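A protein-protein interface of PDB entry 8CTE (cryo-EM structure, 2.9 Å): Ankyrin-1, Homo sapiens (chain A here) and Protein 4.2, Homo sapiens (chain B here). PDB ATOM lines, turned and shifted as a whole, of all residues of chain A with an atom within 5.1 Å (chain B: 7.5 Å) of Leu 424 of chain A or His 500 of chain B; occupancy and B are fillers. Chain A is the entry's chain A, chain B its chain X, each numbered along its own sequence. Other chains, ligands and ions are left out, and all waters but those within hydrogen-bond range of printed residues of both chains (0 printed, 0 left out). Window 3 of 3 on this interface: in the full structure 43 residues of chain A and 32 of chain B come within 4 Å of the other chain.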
ATOM      1  N   LEU A 408       2.346  33.236 -26.221  1.00  0.00           N
ATOM      2  CA  LEU A 408       1.718  33.074 -27.526  1.00  0.00           C
ATOM      3  C   LEU A 408       1.730  34.375 -28.320  1.00  0.00           C
ATOM      4  O   LEU A 408       1.924  34.345 -29.540  1.00  0.00           O
ATOM      5  CB  LEU A 408       0.288  32.558 -27.362  1.00  0.00           C
ATOM      6  CG  LEU A 408      -0.427  32.146 -28.650  1.00  0.00           C
ATOM      7  CD1 LEU A 408       0.381  31.095 -29.390  1.00  0.00           C
ATOM      8  CD2 LEU A 408      -1.819  31.634 -28.343  1.00  0.00           C
ATOM      9  N   ILE A 419       6.812  26.956 -32.230  1.00  0.00           N
ATOM     10  CA  ILE A 419       6.507  27.340 -30.855  1.00  0.00           C
ATOM     11  C   ILE A 419       5.021  27.640 -30.701  1.00  0.00           C
ATOM     12  O   ILE A 419       4.398  27.259 -29.702  1.00  0.00           O
ATOM     13  CB  ILE A 419       7.386  28.530 -30.425  1.00  0.00           C
ATOM     14  CG1 ILE A 419       8.845  28.086 -30.316  1.00  0.00           C
ATOM     15  CG2 ILE A 419       6.899  29.119 -29.107  1.00  0.00           C
ATOM     16  CD1 ILE A 419       9.736  29.069 -29.601  1.00  0.00           C
ATOM     17  N   VAL A 420       4.425  28.314 -31.691  1.00  0.00           N
ATOM     18  CA  VAL A 420       2.984  28.560 -31.672  1.00  0.00           C
ATOM     19  C   VAL A 420       2.222  27.241 -31.674  1.00  0.00           C
ATOM     20  O   VAL A 420       1.250  27.067 -30.928  1.00  0.00           O
ATOM     21  CB  VAL A 420       2.576  29.446 -32.866  1.00  0.00           C
ATOM     22  CG1 VAL A 420       1.063  29.597 -32.931  1.00  0.00           C
ATOM     23  CG2 VAL A 420       3.237  30.805 -32.771  1.00  0.00           C
ATOM     24  N   LYS A 421       2.660  26.293 -32.507  1.00  0.00           N
ATOM     25  CA  LYS A 421       2.000  24.993 -32.572  1.00  0.00           C
ATOM     26  C   LYS A 421       2.096  24.254 -31.245  1.00  0.00           C
ATOM     27  O   LYS A 421       1.107  23.681 -30.775  1.00  0.00           O
ATOM     28  CB  LYS A 421       2.609  24.156 -33.696  1.00  0.00           C
ATOM     29  CG  LYS A 421       1.960  22.792 -33.877  1.00  0.00           C
ATOM     30  CD  LYS A 421       2.713  21.948 -34.892  1.00  0.00           C
ATOM     31  CE  LYS A 421       2.805  22.645 -36.237  1.00  0.00           C
ATOM     32  NZ  LYS A 421       1.461  22.890 -36.826  1.00  0.00           N
ATOM     33  N   ASN A 422       3.275  24.269 -30.619  1.00  0.00           N
ATOM     34  CA  ASN A 422       3.442  23.592 -29.336  1.00  0.00           C
ATOM     35  C   ASN A 422       2.593  24.244 -28.250  1.00  0.00           C
ATOM     36  O   ASN A 422       1.951  23.545 -27.456  1.00  0.00           O
ATOM     37  CB  ASN A 422       4.918  23.583 -28.940  1.00  0.00           C
ATOM     38  CG  ASN A 422       5.265  22.446 -27.997  1.00  0.00           C
ATOM     39  OD1 ASN A 422       4.437  22.008 -27.200  1.00  0.00           O
ATOM     40  ND2 ASN A 422       6.497  21.959 -28.089  1.00  0.00           N
ATOM     41  N   LEU A 423       2.569  25.579 -28.205  1.00  0.00           N
ATOM     42  CA  LEU A 423       1.767  26.273 -27.202  1.00  0.00           C
ATOM     43  C   LEU A 423       0.281  25.990 -27.385  1.00  0.00           C
ATOM     44  O   LEU A 423      -0.441  25.775 -26.406  1.00  0.00           O
ATOM     45  CB  LEU A 423       2.039  27.777 -27.254  1.00  0.00           C
ATOM     46  CG  LEU A 423       3.413  28.247 -26.773  1.00  0.00           C
ATOM     47  CD1 LEU A 423       3.541  29.753 -26.903  1.00  0.00           C
ATOM     48  CD2 LEU A 423       3.659  27.808 -25.342  1.00  0.00           C
ATOM     49  N   LEU A 424      -0.194  25.981 -28.633  1.00  0.00           N
ATOM     50  CA  LEU A 424      -1.602  25.683 -28.873  1.00  0.00           C
ATOM     51  C   LEU A 424      -1.928  24.225 -28.578  1.00  0.00           C
ATOM     52  O   LEU A 424      -3.047  23.916 -28.154  1.00  0.00           O
ATOM     53  CB  LEU A 424      -1.980  26.041 -30.309  1.00  0.00           C
ATOM     54  CG  LEU A 424      -2.011  27.539 -30.618  1.00  0.00           C
ATOM     55  CD1 LEU A 424      -2.467  27.787 -32.042  1.00  0.00           C
ATOM     56  CD2 LEU A 424      -2.909  28.265 -29.634  1.00  0.00           C
ATOM     57  N   GLN A 425      -0.974  23.315 -28.794  1.00  0.00           N
ATOM     58  CA  GLN A 425      -1.185  21.920 -28.427  1.00  0.00           C
ATOM     59  C   GLN A 425      -1.193  21.716 -26.919  1.00  0.00           C
ATOM     60  O   GLN A 425      -1.841  20.782 -26.438  1.00  0.00           O
ATOM     61  CB  GLN A 425      -0.112  21.036 -29.062  1.00  0.00           C
ATOM     62  CG  GLN A 425      -0.321  20.761 -30.540  1.00  0.00           C
ATOM     63  CD  GLN A 425       0.776  19.898 -31.129  1.00  0.00           C
ATOM     64  OE1 GLN A 425       1.902  19.880 -30.632  1.00  0.00           O
ATOM     65  NE2 GLN A 425       0.451  19.171 -32.191  1.00  0.00           N
ATOM     66  N   ARG A 426      -0.491  22.561 -26.167  1.00  0.00           N
ATOM     67  CA  ARG A 426      -0.453  22.452 -24.715  1.00  0.00           C
ATOM     68  C   ARG A 426      -1.597  23.189 -24.031  1.00  0.00           C
ATOM     69  O   ARG A 426      -1.654  23.204 -22.797  1.00  0.00           O
ATOM     70  CB  ARG A 426       0.888  22.964 -24.183  1.00  0.00           C
ATOM     71  CG  ARG A 426       2.071  22.108 -24.597  1.00  0.00           C
ATOM     72  CD  ARG A 426       3.381  22.720 -24.143  1.00  0.00           C
ATOM     73  NE  ARG A 426       3.969  22.002 -23.020  1.00  0.00           N
ATOM     74  CZ  ARG A 426       4.892  21.057 -23.139  1.00  0.00           C
ATOM     75  NH1 ARG A 426       5.359  20.694 -24.321  1.00  0.00           N
ATOM     76  NH2 ARG A 426       5.358  20.463 -22.044  1.00  0.00           N
ATOM     77  N   GLY A 427      -2.504  23.796 -24.790  1.00  0.00           N
ATOM     78  CA  GLY A 427      -3.688  24.407 -24.226  1.00  0.00           C
ATOM     79  C   GLY A 427      -3.656  25.908 -24.047  1.00  0.00           C
ATOM     80  O   GLY A 427      -4.522  26.443 -23.346  1.00  0.00           O
ATOM     81  N   ALA A 428      -2.690  26.605 -24.645  1.00  0.00           N
ATOM     82  CA  ALA A 428      -2.659  28.059 -24.547  1.00  0.00           C
ATOM     83  C   ALA A 428      -3.840  28.667 -25.294  1.00  0.00           C
ATOM     84  O   ALA A 428      -4.171  28.257 -26.409  1.00  0.00           O
ATOM     85  CB  ALA A 428      -1.343  28.605 -25.103  1.00  0.00           C
ATOM     86  N   PRO A 430      -5.713  31.329 -27.462  1.00  0.00           N
ATOM     87  CA  PRO A 430      -5.430  32.438 -28.388  1.00  0.00           C
ATOM     88  C   PRO A 430      -6.338  33.636 -28.183  1.00  0.00           C
ATOM     89  O   PRO A 430      -6.190  34.644 -28.886  1.00  0.00           O
ATOM     90  CB  PRO A 430      -5.639  31.795 -29.765  1.00  0.00           C
ATOM     91  CG  PRO A 430      -6.652  30.727 -29.520  1.00  0.00           C
ATOM     92  CD  PRO A 430      -6.404  30.209 -28.124  1.00  0.00           C
ATOM     93  N   TYR A 455      -2.851  28.790 -38.485  1.00  0.00           N
ATOM     94  CA  TYR A 455      -2.929  27.819 -37.395  1.00  0.00           C
ATOM     95  C   TYR A 455      -3.742  28.365 -36.225  1.00  0.00           C
ATOM     96  O   TYR A 455      -4.520  27.627 -35.601  1.00  0.00           O
ATOM     97  CB  TYR A 455      -1.525  27.420 -36.946  1.00  0.00           C
ATOM     98  CG  TYR A 455      -1.474  26.098 -36.215  1.00  0.00           C
ATOM     99  CD1 TYR A 455      -1.711  24.904 -36.885  1.00  0.00           C
ATOM    100  CD2 TYR A 455      -1.182  26.041 -34.859  1.00  0.00           C
ATOM    101  CE1 TYR A 455      -1.667  23.691 -36.223  1.00  0.00           C
ATOM    102  CE2 TYR A 455      -1.136  24.833 -34.189  1.00  0.00           C
ATOM    103  CZ  TYR A 455      -1.378  23.663 -34.875  1.00  0.00           C
ATOM    104  OH  TYR A 455      -1.331  22.458 -34.211  1.00  0.00           O
ATOM    105  N   LEU A 456      -3.583  29.657 -35.919  1.00  0.00           N
ATOM    106  CA  LEU A 456      -4.385  30.276 -34.867  1.00  0.00           C
ATOM    107  C   LEU A 456      -5.869  30.252 -35.218  1.00  0.00           C
ATOM    108  O   LEU A 456      -6.714  30.004 -34.350  1.00  0.00           O
ATOM    109  CB  LEU A 456      -3.917  31.712 -34.623  1.00  0.00           C
ATOM    110  CG  LEU A 456      -2.571  31.906 -33.923  1.00  0.00           C
ATOM    111  CD1 LEU A 456      -2.139  33.356 -33.997  1.00  0.00           C
ATOM    112  CD2 LEU A 456      -2.657  31.454 -32.480  1.00  0.00           C
ATOM    113  N   ASN A 459      -7.181  26.632 -34.779  1.00  0.00           N
ATOM    114  CA  ASN A 459      -7.277  26.080 -33.420  1.00  0.00           C
ATOM    115  C   ASN A 459      -8.509  26.603 -32.686  1.00  0.00           C
ATOM    116  O   ASN A 459      -9.437  25.841 -32.399  1.00  0.00           O
ATOM    117  CB  ASN A 459      -5.998  26.383 -32.638  1.00  0.00           C
ATOM    118  CG  ASN A 459      -4.896  25.388 -32.925  1.00  0.00           C
ATOM    119  OD1 ASN A 459      -4.603  24.517 -32.107  1.00  0.00           O
ATOM    120  ND2 ASN A 459      -4.287  25.504 -34.098  1.00  0.00           N
ATOM    121  N   LYS A 460      -8.538  27.905 -32.386  1.00  0.00           N
ATOM    122  CA  LYS A 460      -9.688  28.463 -31.680  1.00  0.00           C
ATOM    123  C   LYS A 460     -10.039  29.882 -32.116  1.00  0.00           C
ATOM    124  O   LYS A 460     -10.776  30.570 -31.400  1.00  0.00           O
ATOM    125  CB  LYS A 460      -9.457  28.438 -30.165  1.00  0.00           C
ATOM    126  CG  LYS A 460      -9.975  27.180 -29.489  1.00  0.00           C
ATOM    127  CD  LYS A 460     -11.475  27.037 -29.694  1.00  0.00           C
ATOM    128  CE  LYS A 460     -11.990  25.712 -29.157  1.00  0.00           C
ATOM    129  NZ  LYS A 460     -11.408  24.555 -29.892  1.00  0.00           N
ATOM    130  N   SER B 473      -4.804  14.609 -35.003  1.00  0.00           N
ATOM    131  CA  SER B 473      -4.680  16.065 -34.999  1.00  0.00           C
ATOM    132  C   SER B 473      -5.368  16.757 -33.799  1.00  0.00           C
ATOM    133  O   SER B 473      -4.752  17.621 -33.179  1.00  0.00           O
ATOM    134  CB  SER B 473      -5.204  16.647 -36.321  1.00  0.00           C
ATOM    135  OG  SER B 473      -5.067  18.057 -36.347  1.00  0.00           O
ATOM    136  N   PRO B 474      -6.618  16.406 -33.458  1.00  0.00           N
ATOM    137  CA  PRO B 474      -7.211  17.004 -32.250  1.00  0.00           C
ATOM    138  C   PRO B 474      -6.648  16.441 -30.958  1.00  0.00           C
ATOM    139  O   PRO B 474      -6.967  16.963 -29.883  1.00  0.00           O
ATOM    140  CB  PRO B 474      -8.704  16.685 -32.395  1.00  0.00           C
ATOM    141  CG  PRO B 474      -8.726  15.426 -33.151  1.00  0.00           C
ATOM    142  CD  PRO B 474      -7.607  15.547 -34.146  1.00  0.00           C
ATOM    143  N   LEU B 475      -5.832  15.396 -31.025  1.00  0.00           N
ATOM    144  CA  LEU B 475      -5.276  14.755 -29.844  1.00  0.00           C
ATOM    145  C   LEU B 475      -3.807  15.125 -29.688  1.00  0.00           C
ATOM    146  O   LEU B 475      -3.063  15.184 -30.672  1.00  0.00           O
ATOM    147  CB  LEU B 475      -5.429  13.235 -29.933  1.00  0.00           C
ATOM    148  CG  LEU B 475      -5.048  12.438 -28.687  1.00  0.00           C
ATOM    149  CD1 LEU B 475      -5.958  12.802 -27.529  1.00  0.00           C
ATOM    150  CD2 LEU B 475      -5.094  10.948 -28.969  1.00  0.00           C
ATOM    151  N   TYR B 476      -3.399  15.385 -28.448  1.00  0.00           N
ATOM    152  CA  TYR B 476      -2.017  15.706 -28.119  1.00  0.00           C
ATOM    153  C   TYR B 476      -1.564  14.850 -26.946  1.00  0.00           C
ATOM    154  O   TYR B 476      -2.278  14.723 -25.948  1.00  0.00           O
ATOM    155  CB  TYR B 476      -1.854  17.194 -27.780  1.00  0.00           C
ATOM    156  CG  TYR B 476      -0.471  17.566 -27.299  1.00  0.00           C
ATOM    157  CD1 TYR B 476       0.605  17.598 -28.177  1.00  0.00           C
ATOM    158  CD2 TYR B 476      -0.240  17.891 -25.969  1.00  0.00           C
ATOM    159  CE1 TYR B 476       1.872  17.939 -27.743  1.00  0.00           C
ATOM    160  CE2 TYR B 476       1.023  18.234 -25.525  1.00  0.00           C
ATOM    161  CZ  TYR B 476       2.075  18.257 -26.416  1.00  0.00           C
ATOM    162  OH  TYR B 476       3.334  18.597 -25.981  1.00  0.00           O
ATOM    163  N   LEU B 497      -3.076  13.691 -21.978  1.00  0.00           N
ATOM    164  CA  LEU B 497      -3.876  13.680 -23.195  1.00  0.00           C
ATOM    165  C   LEU B 497      -4.769  14.913 -23.200  1.00  0.00           C
ATOM    166  O   LEU B 497      -5.577  15.102 -22.286  1.00  0.00           O
ATOM    167  CB  LEU B 497      -4.715  12.405 -23.292  1.00  0.00           C
ATOM    168  CG  LEU B 497      -3.939  11.097 -23.456  1.00  0.00           C
ATOM    169  CD1 LEU B 497      -4.890   9.914 -23.520  1.00  0.00           C
ATOM    170  CD2 LEU B 497      -3.065  11.151 -24.697  1.00  0.00           C
ATOM    171  N   VAL B 498      -4.622  15.743 -24.228  1.00  0.00           N
ATOM    172  CA  VAL B 498      -5.402  16.966 -24.377  1.00  0.00           C
ATOM    173  C   VAL B 498      -6.239  16.830 -25.640  1.00  0.00           C
ATOM    174  O   VAL B 498      -5.701  16.614 -26.732  1.00  0.00           O
ATOM    175  CB  VAL B 498      -4.503  18.210 -24.441  1.00  0.00           C
ATOM    176  CG1 VAL B 498      -5.346  19.474 -24.381  1.00  0.00           C
ATOM    177  CG2 VAL B 498      -3.483  18.187 -23.313  1.00  0.00           C
ATOM    178  N   ASN B 499      -7.555  16.957 -25.491  1.00  0.00           N
ATOM    179  CA  ASN B 499      -8.478  16.839 -26.611  1.00  0.00           C
ATOM    180  C   ASN B 499      -8.818  18.231 -27.127  1.00  0.00           C
ATOM    181  O   ASN B 499      -9.361  19.058 -26.387  1.00  0.00           O
ATOM    182  CB  ASN B 499      -9.742  16.092 -26.187  1.00  0.00           C
ATOM    183  CG  ASN B 499     -10.696  15.854 -27.341  1.00  0.00           C
ATOM    184  OD1 ASN B 499     -10.296  15.861 -28.504  1.00  0.00           O
ATOM    185  ND2 ASN B 499     -11.967  15.640 -27.022  1.00  0.00           N
ATOM    186  N   HIS B 500      -8.496  18.490 -28.393  1.00  0.00           N
ATOM    187  CA  HIS B 500      -8.786  19.769 -29.026  1.00  0.00           C
ATOM    188  C   HIS B 500     -10.073  19.752 -29.839  1.00  0.00           C
ATOM    189  O   HIS B 500     -10.406  20.761 -30.468  1.00  0.00           O
ATOM    190  CB  HIS B 500      -7.618  20.194 -29.924  1.00  0.00           C
ATOM    191  CG  HIS B 500      -6.416  20.672 -29.168  1.00  0.00           C
ATOM    192  ND1 HIS B 500      -5.830  19.940 -28.158  1.00  0.00           N
ATOM    193  CD2 HIS B 500      -5.689  21.809 -29.278  1.00  0.00           C
ATOM    194  CE1 HIS B 500      -4.796  20.606 -27.677  1.00  0.00           C
ATOM    195  NE2 HIS B 500      -4.688  21.743 -28.340  1.00  0.00           N
ATOM    196  N   SER B 501     -10.801  18.640 -29.841  1.00  0.00           N
ATOM    197  CA  SER B 501     -12.030  18.538 -30.608  1.00  0.00           C
ATOM    198  C   SER B 501     -13.218  19.041 -29.791  1.00  0.00           C
ATOM    199  O   SER B 501     -13.165  19.163 -28.564  1.00  0.00           O
ATOM    200  CB  SER B 501     -12.261  17.095 -31.055  1.00  0.00           C
ATOM    201  OG  SER B 501     -13.448  16.983 -31.820  1.00  0.00           O
ATOM    202  N   GLU B 502     -14.309  19.338 -30.497  1.00  0.00           N
ATOM    203  CA  GLU B 502     -15.544  19.787 -29.869  1.00  0.00           C
ATOM    204  C   GLU B 502     -16.432  18.638 -29.413  1.00  0.00           C
ATOM    205  O   GLU B 502     -17.487  18.890 -28.820  1.00  0.00           O
ATOM    206  CB  GLU B 502     -16.329  20.687 -30.831  1.00  0.00           C
ATOM    207  CG  GLU B 502     -15.655  22.018 -31.132  1.00  0.00           C
ATOM    208  CD  GLU B 502     -15.697  22.973 -29.954  1.00  0.00           C
ATOM    209  OE1 GLU B 502     -16.558  22.792 -29.067  1.00  0.00           O
ATOM    210  OE2 GLU B 502     -14.868  23.907 -29.916  1.00  0.00           O
ATOM    211  N   GLN B 503     -16.036  17.395 -29.670  1.00  0.00           N
ATOM    212  CA  GLN B 503     -16.804  16.219 -29.294  1.00  0.00           C
ATOM    213  C   GLN B 503     -15.929  15.280 -28.476  1.00  0.00           C
ATOM    214  O   GLN B 503     -14.707  15.247 -28.654  1.00  0.00           O
ATOM    215  CB  GLN B 503     -17.344  15.498 -30.535  1.00  0.00           C
ATOM    216  CG  GLN B 503     -16.301  15.269 -31.617  1.00  0.00           C
ATOM    217  CD  GLN B 503     -16.901  14.731 -32.901  1.00  0.00           C
ATOM    218  OE1 GLN B 503     -18.044  14.275 -32.924  1.00  0.00           O
ATOM    219  NE2 GLN B 503     -16.131  14.788 -33.983  1.00  0.00           N
ATOM    220  N   LYS B 505     -14.097  11.937 -27.093  1.00  0.00           N
ATOM    221  CA  LYS B 505     -13.303  10.999 -27.867  1.00  0.00           C
ATOM    222  C   LYS B 505     -12.988   9.764 -27.034  1.00  0.00           C
ATOM    223  O   LYS B 505     -12.786   9.847 -25.820  1.00  0.00           O
ATOM    224  CB  LYS B 505     -12.005  11.661 -28.346  1.00  0.00           C
ATOM    225  CG  LYS B 505     -11.464  11.116 -29.652  1.00  0.00           C
ATOM    226  CD  LYS B 505     -10.471  12.089 -30.261  1.00  0.00           C
ATOM    227  CE  LYS B 505     -11.132  13.416 -30.589  1.00  0.00           C
ATOM    228  NZ  LYS B 505     -12.253  13.252 -31.555  1.00  0.00           N
ATOM    229  N   SER B 536     -13.124  13.984 -22.424  1.00  0.00           N
ATOM    230  CA  SER B 536     -14.127  15.019 -22.609  1.00  0.00           C
ATOM    231  C   SER B 536     -13.639  16.057 -23.613  1.00  0.00           C
ATOM    232  O   SER B 536     -12.436  16.259 -23.798  1.00  0.00           O
ATOM    233  CB  SER B 536     -14.454  15.692 -21.276  1.00  0.00           C
ATOM    234  OG  SER B 536     -14.919  14.747 -20.328  1.00  0.00           O
ATOM    235  N   ALA B 537     -14.592  16.711 -24.270  1.00  0.00           N
ATOM    236  CA  ALA B 537     -14.254  17.712 -25.272  1.00  0.00           C
ATOM    237  C   ALA B 537     -13.613  18.929 -24.617  1.00  0.00           C
ATOM    238  O   ALA B 537     -14.137  19.470 -23.639  1.00  0.00           O
ATOM    239  CB  ALA B 537     -15.505  18.122 -26.048  1.00  0.00           C
ATOM    240  N   ASN B 538     -12.473  19.354 -25.171  1.00  0.00           N
ATOM    241  CA  ASN B 538     -11.730  20.526 -24.701  1.00  0.00           C
ATOM    242  C   ASN B 538     -11.363  20.401 -23.222  1.00  0.00           C
ATOM    243  O   ASN B 538     -11.618  21.297 -22.413  1.00  0.00           O
ATOM    244  CB  ASN B 538     -12.511  21.816 -24.967  1.00  0.00           C
ATOM    245  CG  ASN B 538     -12.932  21.954 -26.416  1.00  0.00           C
ATOM    246  OD1 ASN B 538     -12.177  22.451 -27.250  1.00  0.00           O
ATOM    247  ND2 ASN B 538     -14.146  21.510 -26.724  1.00  0.00           N
ATOM    248  N   LEU B 539     -10.754  19.271 -22.869  1.00  0.00           N
ATOM    249  CA  LEU B 539     -10.349  19.008 -21.496  1.00  0.00           C
ATOM    250  C   LEU B 539      -8.999  18.306 -21.485  1.00  0.00           C
ATOM    251  O   LEU B 539      -8.729  17.451 -22.334  1.00  0.00           O
ATOM    252  CB  LEU B 539     -11.391  18.158 -20.758  1.00  0.00           C
ATOM    253  CG  LEU B 539     -11.151  17.940 -19.263  1.00  0.00           C
ATOM    254  CD1 LEU B 539     -11.087  19.272 -18.532  1.00  0.00           C
ATOM    255  CD2 LEU B 539     -12.228  17.050 -18.665  1.00  0.00           C
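The side-chain amide oxygen (OD1) of Asn 422 of chain A lies within hydrogen-bond range of the guanidinium group (NH1) of Arg 426 of chain A, at 3.3 Å.
N of His 500 of chain B lies within hydrogen-bond range of O of Pro 474 of chain B, 2.6 Å away.
N of Val 498 of chain B sits at hydrogen-bond distance from O of Tyr 476 of chain B (3.1 Å).
The backbone carbonyl oxygen (O) of Asn 499 of chain B lies close to the backbone NH (N) of Asn 538 of chain B (3.4 Å).
The backbone carbonyl oxygen of Ser 501 of chain B sits at hydrogen-bond distance from the side-chain amide nitrogen of Asn 538 of chain B, at 3.1 Å.
Of the 16 printed residues of chain B, 4 touch a printed residue of chain A.
Hydrophobic or aromatic side chains of chain B within 4 Å of the printed part of chain A: Tyr 476 and His 500.
Among the printed residues, Asp or Glu carboxylates within 4 Å of a Lys or Arg side-chain nitrogen of the other chain: Lys 460 of chain A with Glu 502 of chain B.
Among the printed residues, pairs that only touch across the chains: Gln 425 of chain A with His 500 of chain B, Gln 425 of chain A with Tyr 476 of chain B, Asn 422 of chain A with Tyr 476 of chain B and Lys 460 of chain A with His 500 of chain B.
O of Leu 424 of chain A lies within hydrogen-bond range of NE2 of His 500 of chain B, 2.7 Å away.
NH1 of Arg 426 of chain A is in hydrogen-bond range of OH of Tyr 476 of chain B (3.4 Å).
OE2 of Glu 502 of chain B is in salt-bridge range of NZ of Lys 460 of chain A (3.5 Å).
OD1 of Asn 538 of chain B sits at hydrogen-bond distance from NZ of Lys 460 of chain A (3.5 Å).
Ile 419 of chain A touches none of the printed residues of chain B.
Of the printed residues of chain B, Leu 424 of chain A touches His 500 (2.7 Å).
Leu 475 of chain B touches none of the printed residues of chain A.
Printed residues of chain A within 4 Å of Tyr 476 of chain B: Asn 422, Gln 425 and Arg 426.
His 500 of chain B touches three residues of chain A.
Printed residues of chain A within 4 Å of Asn 538 of chain B: Lys 460 (3.5 Å).
The nearest residue of chain A that does not touch His 500 of chain B is Asn 459 of chain A (4.1 Å).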
